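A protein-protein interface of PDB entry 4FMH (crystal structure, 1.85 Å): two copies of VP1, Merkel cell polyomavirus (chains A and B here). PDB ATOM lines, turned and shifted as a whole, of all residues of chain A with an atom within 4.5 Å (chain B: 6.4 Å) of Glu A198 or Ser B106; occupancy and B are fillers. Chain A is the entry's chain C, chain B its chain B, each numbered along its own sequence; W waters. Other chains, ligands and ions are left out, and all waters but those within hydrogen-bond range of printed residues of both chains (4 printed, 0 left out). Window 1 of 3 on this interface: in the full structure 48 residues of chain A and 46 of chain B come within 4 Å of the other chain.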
ATOM      1  N   LEU A  67       0.913   3.001 -11.372  1.00  0.00           N
ATOM      2  CA  LEU A  67       0.330   3.313 -12.676  1.00  0.00           C
ATOM      3  C   LEU A  67      -0.298   2.081 -13.339  1.00  0.00           C
ATOM      4  O   LEU A  67       0.341   1.433 -14.179  1.00  0.00           O
ATOM      5  CB  LEU A  67       1.374   3.953 -13.601  1.00  0.00           C
ATOM      6  CG  LEU A  67       2.099   5.216 -13.119  1.00  0.00           C
ATOM      7  CD1 LEU A  67       3.271   5.579 -14.053  1.00  0.00           C
ATOM      8  CD2 LEU A  67       1.143   6.379 -12.975  1.00  0.00           C
ATOM      9  N   LEU A 147      -4.242  11.824 -22.851  1.00  0.00           N
ATOM     10  CA  LEU A 147      -4.786  12.979 -22.136  1.00  0.00           C
ATOM     11  C   LEU A 147      -4.520  12.763 -20.652  1.00  0.00           C
ATOM     12  O   LEU A 147      -4.797  11.686 -20.125  1.00  0.00           O
ATOM     13  CB  LEU A 147      -6.292  13.149 -22.395  1.00  0.00           C
ATOM     14  CG  LEU A 147      -6.972  14.409 -21.840  1.00  0.00           C
ATOM     15  CD1 LEU A 147      -8.133  14.842 -22.724  1.00  0.00           C
ATOM     16  CD2 LEU A 147      -7.449  14.229 -20.399  1.00  0.00           C
ATOM     17  N   VAL A 148      -3.974  13.778 -19.984  1.00  0.00           N
ATOM     18  CA  VAL A 148      -3.647  13.645 -18.558  1.00  0.00           C
ATOM     19  C   VAL A 148      -4.315  14.711 -17.704  1.00  0.00           C
ATOM     20  O   VAL A 148      -4.631  15.801 -18.183  1.00  0.00           O
ATOM     21  CB  VAL A 148      -2.101  13.664 -18.305  1.00  0.00           C
ATOM     22  CG1 VAL A 148      -1.452  12.435 -18.913  1.00  0.00           C
ATOM     23  CG2 VAL A 148      -1.459  14.953 -18.855  1.00  0.00           C
ATOM     24  N   LEU A 149      -4.513  14.385 -16.433  1.00  0.00           N
ATOM     25  CA  LEU A 149      -5.053  15.324 -15.456  1.00  0.00           C
ATOM     26  C   LEU A 149      -4.136  16.542 -15.281  1.00  0.00           C
ATOM     27  O   LEU A 149      -4.611  17.679 -15.170  1.00  0.00           O
ATOM     28  CB  LEU A 149      -5.231  14.613 -14.107  1.00  0.00           C
ATOM     29  CG  LEU A 149      -5.998  15.390 -13.026  1.00  0.00           C
ATOM     30  CD1 LEU A 149      -7.494  15.392 -13.309  1.00  0.00           C
ATOM     31  CD2 LEU A 149      -5.721  14.801 -11.635  1.00  0.00           C
ATOM     32  N   TYR A 155       6.343  11.493 -15.518  1.00  0.00           N
ATOM     33  CA  TYR A 155       6.217  10.035 -15.572  1.00  0.00           C
ATOM     34  C   TYR A 155       7.593   9.373 -15.716  1.00  0.00           C
ATOM     35  O   TYR A 155       8.537  10.012 -16.194  1.00  0.00           O
ATOM     36  CB  TYR A 155       5.264   9.623 -16.699  1.00  0.00           C
ATOM     37  CG  TYR A 155       3.815   9.967 -16.411  1.00  0.00           C
ATOM     38  CD1 TYR A 155       3.041   9.163 -15.569  1.00  0.00           C
ATOM     39  CD2 TYR A 155       3.216  11.092 -16.980  1.00  0.00           C
ATOM     40  CE1 TYR A 155       1.696   9.477 -15.296  1.00  0.00           C
ATOM     41  CE2 TYR A 155       1.881  11.412 -16.718  1.00  0.00           C
ATOM     42  CZ  TYR A 155       1.131  10.599 -15.872  1.00  0.00           C
ATOM     43  OH  TYR A 155      -0.183  10.909 -15.606  1.00  0.00           O
ATOM     44  N   PRO A 196      -0.148   3.233 -19.352  1.00  0.00           N
ATOM     45  CA  PRO A 196      -0.924   3.619 -18.174  1.00  0.00           C
ATOM     46  C   PRO A 196      -2.343   4.099 -18.494  1.00  0.00           C
ATOM     47  O   PRO A 196      -2.557   4.924 -19.391  1.00  0.00           O
ATOM     48  CB  PRO A 196      -0.089   4.743 -17.550  1.00  0.00           C
ATOM     49  CG  PRO A 196       1.307   4.479 -18.036  1.00  0.00           C
ATOM     50  CD  PRO A 196       1.124   3.978 -19.437  1.00  0.00           C
ATOM     51  N   ILE A 197      -3.299   3.557 -17.757  1.00  0.00           N
ATOM     52  CA  ILE A 197      -4.706   3.929 -17.893  1.00  0.00           C
ATOM     53  C   ILE A 197      -4.926   5.438 -17.676  1.00  0.00           C
ATOM     54  O   ILE A 197      -5.704   6.058 -18.396  1.00  0.00           O
ATOM     55  CB  ILE A 197      -5.581   3.083 -16.942  1.00  0.00           C
ATOM     56  CG1 ILE A 197      -5.569   1.618 -17.392  1.00  0.00           C
ATOM     57  CG2 ILE A 197      -7.011   3.630 -16.866  1.00  0.00           C
ATOM     58  CD1 ILE A 197      -5.932   0.636 -16.282  1.00  0.00           C
ATOM     59  N   GLU A 198      -4.211   6.041 -16.727  1.00  0.00           N
ATOM     60  CA  GLU A 198      -4.415   7.469 -16.435  1.00  0.00           C
ATOM     61  C   GLU A 198      -3.867   8.411 -17.525  1.00  0.00           C
ATOM     62  O   GLU A 198      -4.129   9.612 -17.503  1.00  0.00           O
ATOM     63  CB  GLU A 198      -3.852   7.833 -15.057  1.00  0.00           C
ATOM     64  CG  GLU A 198      -2.330   8.064 -15.017  1.00  0.00           C
ATOM     65  CD  GLU A 198      -1.862   8.578 -13.662  1.00  0.00           C
ATOM     66  OE1 GLU A 198      -2.288   8.021 -12.630  1.00  0.00           O
ATOM     67  OE2 GLU A 198      -1.072   9.539 -13.629  1.00  0.00           O
ATOM     68  N   VAL A 199      -3.113   7.854 -18.467  1.00  0.00           N
ATOM     69  CA  VAL A 199      -2.548   8.621 -19.576  1.00  0.00           C
ATOM     70  C   VAL A 199      -3.276   8.361 -20.903  1.00  0.00           C
ATOM     71  O   VAL A 199      -3.489   9.293 -21.689  1.00  0.00           O
ATOM     72  CB  VAL A 199      -1.038   8.313 -19.730  1.00  0.00           C
ATOM     73  CG1 VAL A 199      -0.453   9.012 -20.947  1.00  0.00           C
ATOM     74  CG2 VAL A 199      -0.282   8.707 -18.454  1.00  0.00           C
ATOM     75  N   TRP A 200      -3.670   7.105 -21.135  1.00  0.00           N
ATOM     76  CA  TRP A 200      -4.209   6.685 -22.432  1.00  0.00           C
ATOM     77  C   TRP A 200      -5.665   6.232 -22.328  1.00  0.00           C
ATOM     78  O   TRP A 200      -6.029   5.503 -21.402  1.00  0.00           O
ATOM     79  CB  TRP A 200      -3.368   5.544 -23.023  1.00  0.00           C
ATOM     80  CG  TRP A 200      -1.908   5.865 -23.167  1.00  0.00           C
ATOM     81  CD1 TRP A 200      -0.897   5.442 -22.356  1.00  0.00           C
ATOM     82  CD2 TRP A 200      -1.301   6.686 -24.176  1.00  0.00           C
ATOM     83  NE1 TRP A 200       0.308   5.947 -22.799  1.00  0.00           N
ATOM     84  CE2 TRP A 200       0.087   6.714 -23.911  1.00  0.00           C
ATOM     85  CE3 TRP A 200      -1.795   7.397 -25.277  1.00  0.00           C
ATOM     86  CZ2 TRP A 200       0.991   7.424 -24.711  1.00  0.00           C
ATOM     87  CZ3 TRP A 200      -0.901   8.114 -26.073  1.00  0.00           C
ATOM     88  CH2 TRP A 200       0.481   8.117 -25.787  1.00  0.00           C
ATOM     89  N   VAL B 102     -13.789  12.256 -24.428  1.00  0.00           N
ATOM     90  CA  VAL B 102     -12.420  11.758 -24.571  1.00  0.00           C
ATOM     91  C   VAL B 102     -11.636  11.988 -23.283  1.00  0.00           C
ATOM     92  O   VAL B 102     -11.816  13.010 -22.619  1.00  0.00           O
ATOM     93  CB  VAL B 102     -11.711  12.461 -25.768  1.00  0.00           C
ATOM     94  CG1 VAL B 102     -10.226  12.065 -25.871  1.00  0.00           C
ATOM     95  CG2 VAL B 102     -12.445  12.146 -27.074  1.00  0.00           C
ATOM     96  N   GLY B 103     -10.761  11.046 -22.933  1.00  0.00           N
ATOM     97  CA  GLY B 103      -9.897  11.215 -21.762  1.00  0.00           C
ATOM     98  C   GLY B 103     -10.541  10.828 -20.445  1.00  0.00           C
ATOM     99  O   GLY B 103     -10.109  11.266 -19.366  1.00  0.00           O
ATOM    100  N   ILE B 104     -11.570   9.990 -20.519  1.00  0.00           N
ATOM    101  CA  ILE B 104     -12.256   9.550 -19.309  1.00  0.00           C
ATOM    102  C   ILE B 104     -11.294   8.833 -18.346  1.00  0.00           C
ATOM    103  O   ILE B 104     -11.325   9.075 -17.131  1.00  0.00           O
ATOM    104  CB  ILE B 104     -13.511   8.693 -19.636  1.00  0.00           C
ATOM    105  CG1 ILE B 104     -14.655   9.592 -20.128  1.00  0.00           C
ATOM    106  CG2 ILE B 104     -13.969   7.934 -18.406  1.00  0.00           C
ATOM    107  CD1 ILE B 104     -15.744   8.840 -20.918  1.00  0.00           C
ATOM    108  N   SER B 105     -10.424   7.988 -18.901  1.00  0.00           N
ATOM    109  CA  SER B 105      -9.452   7.227 -18.118  1.00  0.00           C
ATOM    110  C   SER B 105      -8.506   8.102 -17.276  1.00  0.00           C
ATOM    111  O   SER B 105      -8.029   7.666 -16.230  1.00  0.00           O
ATOM    112  CB  SER B 105      -8.629   6.310 -19.032  1.00  0.00           C
ATOM    113  OG  SER B 105      -7.803   7.071 -19.889  1.00  0.00           O
ATOM    114  N   SER B 106      -8.250   9.330 -17.725  1.00  0.00           N
ATOM    115  CA  SER B 106      -7.402  10.256 -16.972  1.00  0.00           C
ATOM    116  C   SER B 106      -7.925  10.511 -15.559  1.00  0.00           C
ATOM    117  O   SER B 106      -7.165  10.916 -14.686  1.00  0.00           O
ATOM    118  CB  SER B 106      -7.258  11.593 -17.711  1.00  0.00           C
ATOM    119  OG  SER B 106      -8.425  12.387 -17.549  1.00  0.00           O
ATOM    120  N   LEU B 107      -9.223  10.293 -15.343  1.00  0.00           N
ATOM    121  CA  LEU B 107      -9.829  10.577 -14.044  1.00  0.00           C
ATOM    122  C   LEU B 107      -9.551   9.529 -12.955  1.00  0.00           C
ATOM    123  O   LEU B 107      -9.966   9.708 -11.803  1.00  0.00           O
ATOM    124  CB  LEU B 107     -11.336  10.859 -14.174  1.00  0.00           C
ATOM    125  CG  LEU B 107     -11.755  11.978 -15.148  1.00  0.00           C
ATOM    126  CD1 LEU B 107     -13.281  12.153 -15.173  1.00  0.00           C
ATOM    127  CD2 LEU B 107     -11.050  13.303 -14.823  1.00  0.00           C
ATOM    128  N   ILE B 108      -8.838   8.454 -13.292  1.00  0.00           N
ATOM    129  CA  ILE B 108      -8.398   7.509 -12.246  1.00  0.00           C
ATOM    130  C   ILE B 108      -7.196   8.040 -11.448  1.00  0.00           C
ATOM    131  O   ILE B 108      -6.806   7.444 -10.444  1.00  0.00           O
ATOM    132  CB  ILE B 108      -8.074   6.084 -12.770  1.00  0.00           C
ATOM    133  CG1 ILE B 108      -6.754   6.065 -13.542  1.00  0.00           C
ATOM    134  CG2 ILE B 108      -9.244   5.504 -13.585  1.00  0.00           C
ATOM    135  CD1 ILE B 108      -6.042   4.699 -13.482  1.00  0.00           C
ATOM    136  N   ASN B 109      -6.612   9.146 -11.909  1.00  0.00           N
ATOM    137  CA  ASN B 109      -5.490   9.778 -11.216  1.00  0.00           C
ATOM    138  C   ASN B 109      -5.918  10.297  -9.836  1.00  0.00           C
ATOM    139  O   ASN B 109      -6.688  11.249  -9.735  1.00  0.00           O
ATOM    140  CB  ASN B 109      -4.893  10.904 -12.076  1.00  0.00           C
ATOM    141  CG  ASN B 109      -3.652  11.532 -11.454  1.00  0.00           C
ATOM    142  OD1 ASN B 109      -3.434  11.462 -10.237  1.00  0.00           O
ATOM    143  ND2 ASN B 109      -2.832  12.157 -12.289  1.00  0.00           N
ATOM    144  N   VAL B 110      -5.432   9.648  -8.779  1.00  0.00           N
ATOM    145  CA  VAL B 110      -5.740  10.066  -7.401  1.00  0.00           C
ATOM    146  C   VAL B 110      -4.483  10.519  -6.657  1.00  0.00           C
ATOM    147  O   VAL B 110      -4.392  10.416  -5.434  1.00  0.00           O
ATOM    148  CB  VAL B 110      -6.494   8.968  -6.600  1.00  0.00           C
ATOM    149  CG1 VAL B 110      -7.929   8.764  -7.159  1.00  0.00           C
ATOM    150  CG2 VAL B 110      -5.695   7.651  -6.567  1.00  0.00           C
ATOM    151  N   HIS B 111      -3.526  11.048  -7.412  1.00  0.00           N
ATOM    152  CA  HIS B 111      -2.226  11.421  -6.866  1.00  0.00           C
ATOM    153  C   HIS B 111      -1.722  12.730  -7.474  1.00  0.00           C
ATOM    154  O   HIS B 111      -0.511  12.931  -7.620  1.00  0.00           O
ATOM    155  CB  HIS B 111      -1.209  10.290  -7.061  1.00  0.00           C
ATOM    156  CG  HIS B 111      -1.095   9.831  -8.478  1.00  0.00           C
ATOM    157  ND1 HIS B 111      -0.292  10.468  -9.402  1.00  0.00           N
ATOM    158  CD2 HIS B 111      -1.712   8.826  -9.144  1.00  0.00           C
ATOM    159  CE1 HIS B 111      -0.409   9.863 -10.571  1.00  0.00           C
ATOM    160  NE2 HIS B 111      -1.268   8.867 -10.443  1.00  0.00           N
ATOM    161  N   HIS B 272     -13.678  20.903 -13.619  1.00  0.00           N
ATOM    162  CA  HIS B 272     -12.840  20.322 -14.664  1.00  0.00           C
ATOM    163  C   HIS B 272     -13.757  19.805 -15.762  1.00  0.00           C
ATOM    164  O   HIS B 272     -14.859  19.320 -15.486  1.00  0.00           O
ATOM    165  CB  HIS B 272     -12.012  19.176 -14.062  1.00  0.00           C
ATOM    166  CG  HIS B 272     -11.065  18.507 -15.017  1.00  0.00           C
ATOM    167  ND1 HIS B 272     -10.272  19.199 -15.908  1.00  0.00           N
ATOM    168  CD2 HIS B 272     -10.744  17.199 -15.172  1.00  0.00           C
ATOM    169  CE1 HIS B 272      -9.532  18.345 -16.593  1.00  0.00           C
ATOM    170  NE2 HIS B 272      -9.798  17.125 -16.165  1.00  0.00           N
ATOM    171  N   LEU B 274     -13.834  17.714 -19.869  1.00  0.00           N
ATOM    172  CA  LEU B 274     -13.122  16.872 -20.833  1.00  0.00           C
ATOM    173  C   LEU B 274     -13.547  17.209 -22.268  1.00  0.00           C
ATOM    174  O   LEU B 274     -14.634  17.764 -22.468  1.00  0.00           O
ATOM    175  CB  LEU B 274     -13.372  15.386 -20.526  1.00  0.00           C
ATOM    176  CG  LEU B 274     -12.724  14.824 -19.256  1.00  0.00           C
ATOM    177  CD1 LEU B 274     -13.207  13.387 -19.038  1.00  0.00           C
ATOM    178  CD2 LEU B 274     -11.197  14.853 -19.366  1.00  0.00           C
HETATM  179  O   HOH W   1      -4.439  11.422 -15.504  1.00  0.00           O
HETATM  180  O   HOH W   2      -1.769  13.368 -14.801  1.00  0.00           O
HETATM  181  O   HOH W   3      -6.903  17.129 -18.031  1.00  0.00           O
HETATM  182  O   HOH W   4      -6.947   9.725 -20.856  1.00  0.00           O
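The backbone carbonyl oxygen of Ile A197 is in hydrogen-bond range of the side-chain hydroxyl of Ser B105, at 2.8 Å. OG of Ser B105 sits at hydrogen-bond distance from O of Trp A200 (2.8 Å). The side-chain amide nitrogen (ND2) of Asn B109 is in hydrogen-bond range of the side-chain carboxylate (OE2) of Glu A198, 3.4 Å away. A ring nitrogen (NE2) of His B111 sits at hydrogen-bond distance from the side-chain carboxylate (OE1) of Glu A198, at 2.6 Å.
OG of Ser B106 sits at hydrogen-bond distance from O of Gly B103, 2.7 Å away. N of His B111 sits at hydrogen-bond distance from OD1 of Asn B109, at 2.9 Å. The backbone NH (N) of Leu A147 is in hydrogen-bond range of the backbone carbonyl oxygen (O) of Val A199, 2.9 Å away. OH of Tyr A155 is in hydrogen-bond range of OE2 of Glu A198 (2.6 Å).
Among the printed residues, pairs that only touch across the chains: Leu A147 with Ser B106, Leu A147 with Leu B274, Leu A149 with Asn B109, Ile A197 with Ile B108, Glu A198 with Ser B105, Glu A198 with Ser B106 and Glu A198 with Ile B108.
Printed residues of chain B within 4 Å of Leu A147: Ser B106 and Leu B274. Of the printed residues of chain B, Leu A149 touches Asn B109. Pro A196 touches none of the printed residues of chain B. Printed residues of chain B within 4 Å of Ile A197: Ser B105 and Ile B108. Of the printed residues of chain B, Glu A198 touches Ser B105, Ser B106, Ile B108, Asn B109 and His B111. Gly B103 touches none of the printed residues of chain A. Of the printed residues of chain A, Ser B105 touches Ile A197, Glu A198 and Trp A200. The nearest residue of chain B that does not touch Glu A198 is Val B110 (5.2 Å).
Printed residues of chain B that touch a printed residue of chain A: Ser B105, Ser B106, Ile B108, Asn B109, His B111 and Leu B274. Along chain B the printed residues that touch a printed residue of chain A span positions 105 to 274. Among the printed residues, 11 pairs touch across the chains. Among the printed residues, no Asp or Glu carboxylate lies within 4 Å of a Lys or Arg side-chain nitrogen of the other chain.
No position is printed for both chains. Of the 11 pairs that touch across the chains among the printed residues, none has its exchanged pair printed and touching as well.
Water W3 lies within hydrogen-bond range of O of Val A148 (2.6 Å) and NE2 of His B272 (3.4 Å). Water W1 lies within hydrogen-bond range of the backbone carbonyl oxygen of Glu A198 (2.7 Å), the backbone carbonyl oxygen of Ser B106 (2.9 Å) and the backbone NH of Leu A149 (3.1 Å). Water W4 lies within hydrogen-bond range of the side-chain hydroxyl (OG) of Ser B105 (3.0 Å), the backbone carbonyl oxygen (O) of Leu A147 (3.0 Å) and the backbone NH (N) of Ser B106 (3.4 Å). Water W2 lies within hydrogen-bond range of the side-chain amide nitrogen of Asn B109, the side-chain hydroxyl of Tyr A155 and the backbone NH of Leu A149.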
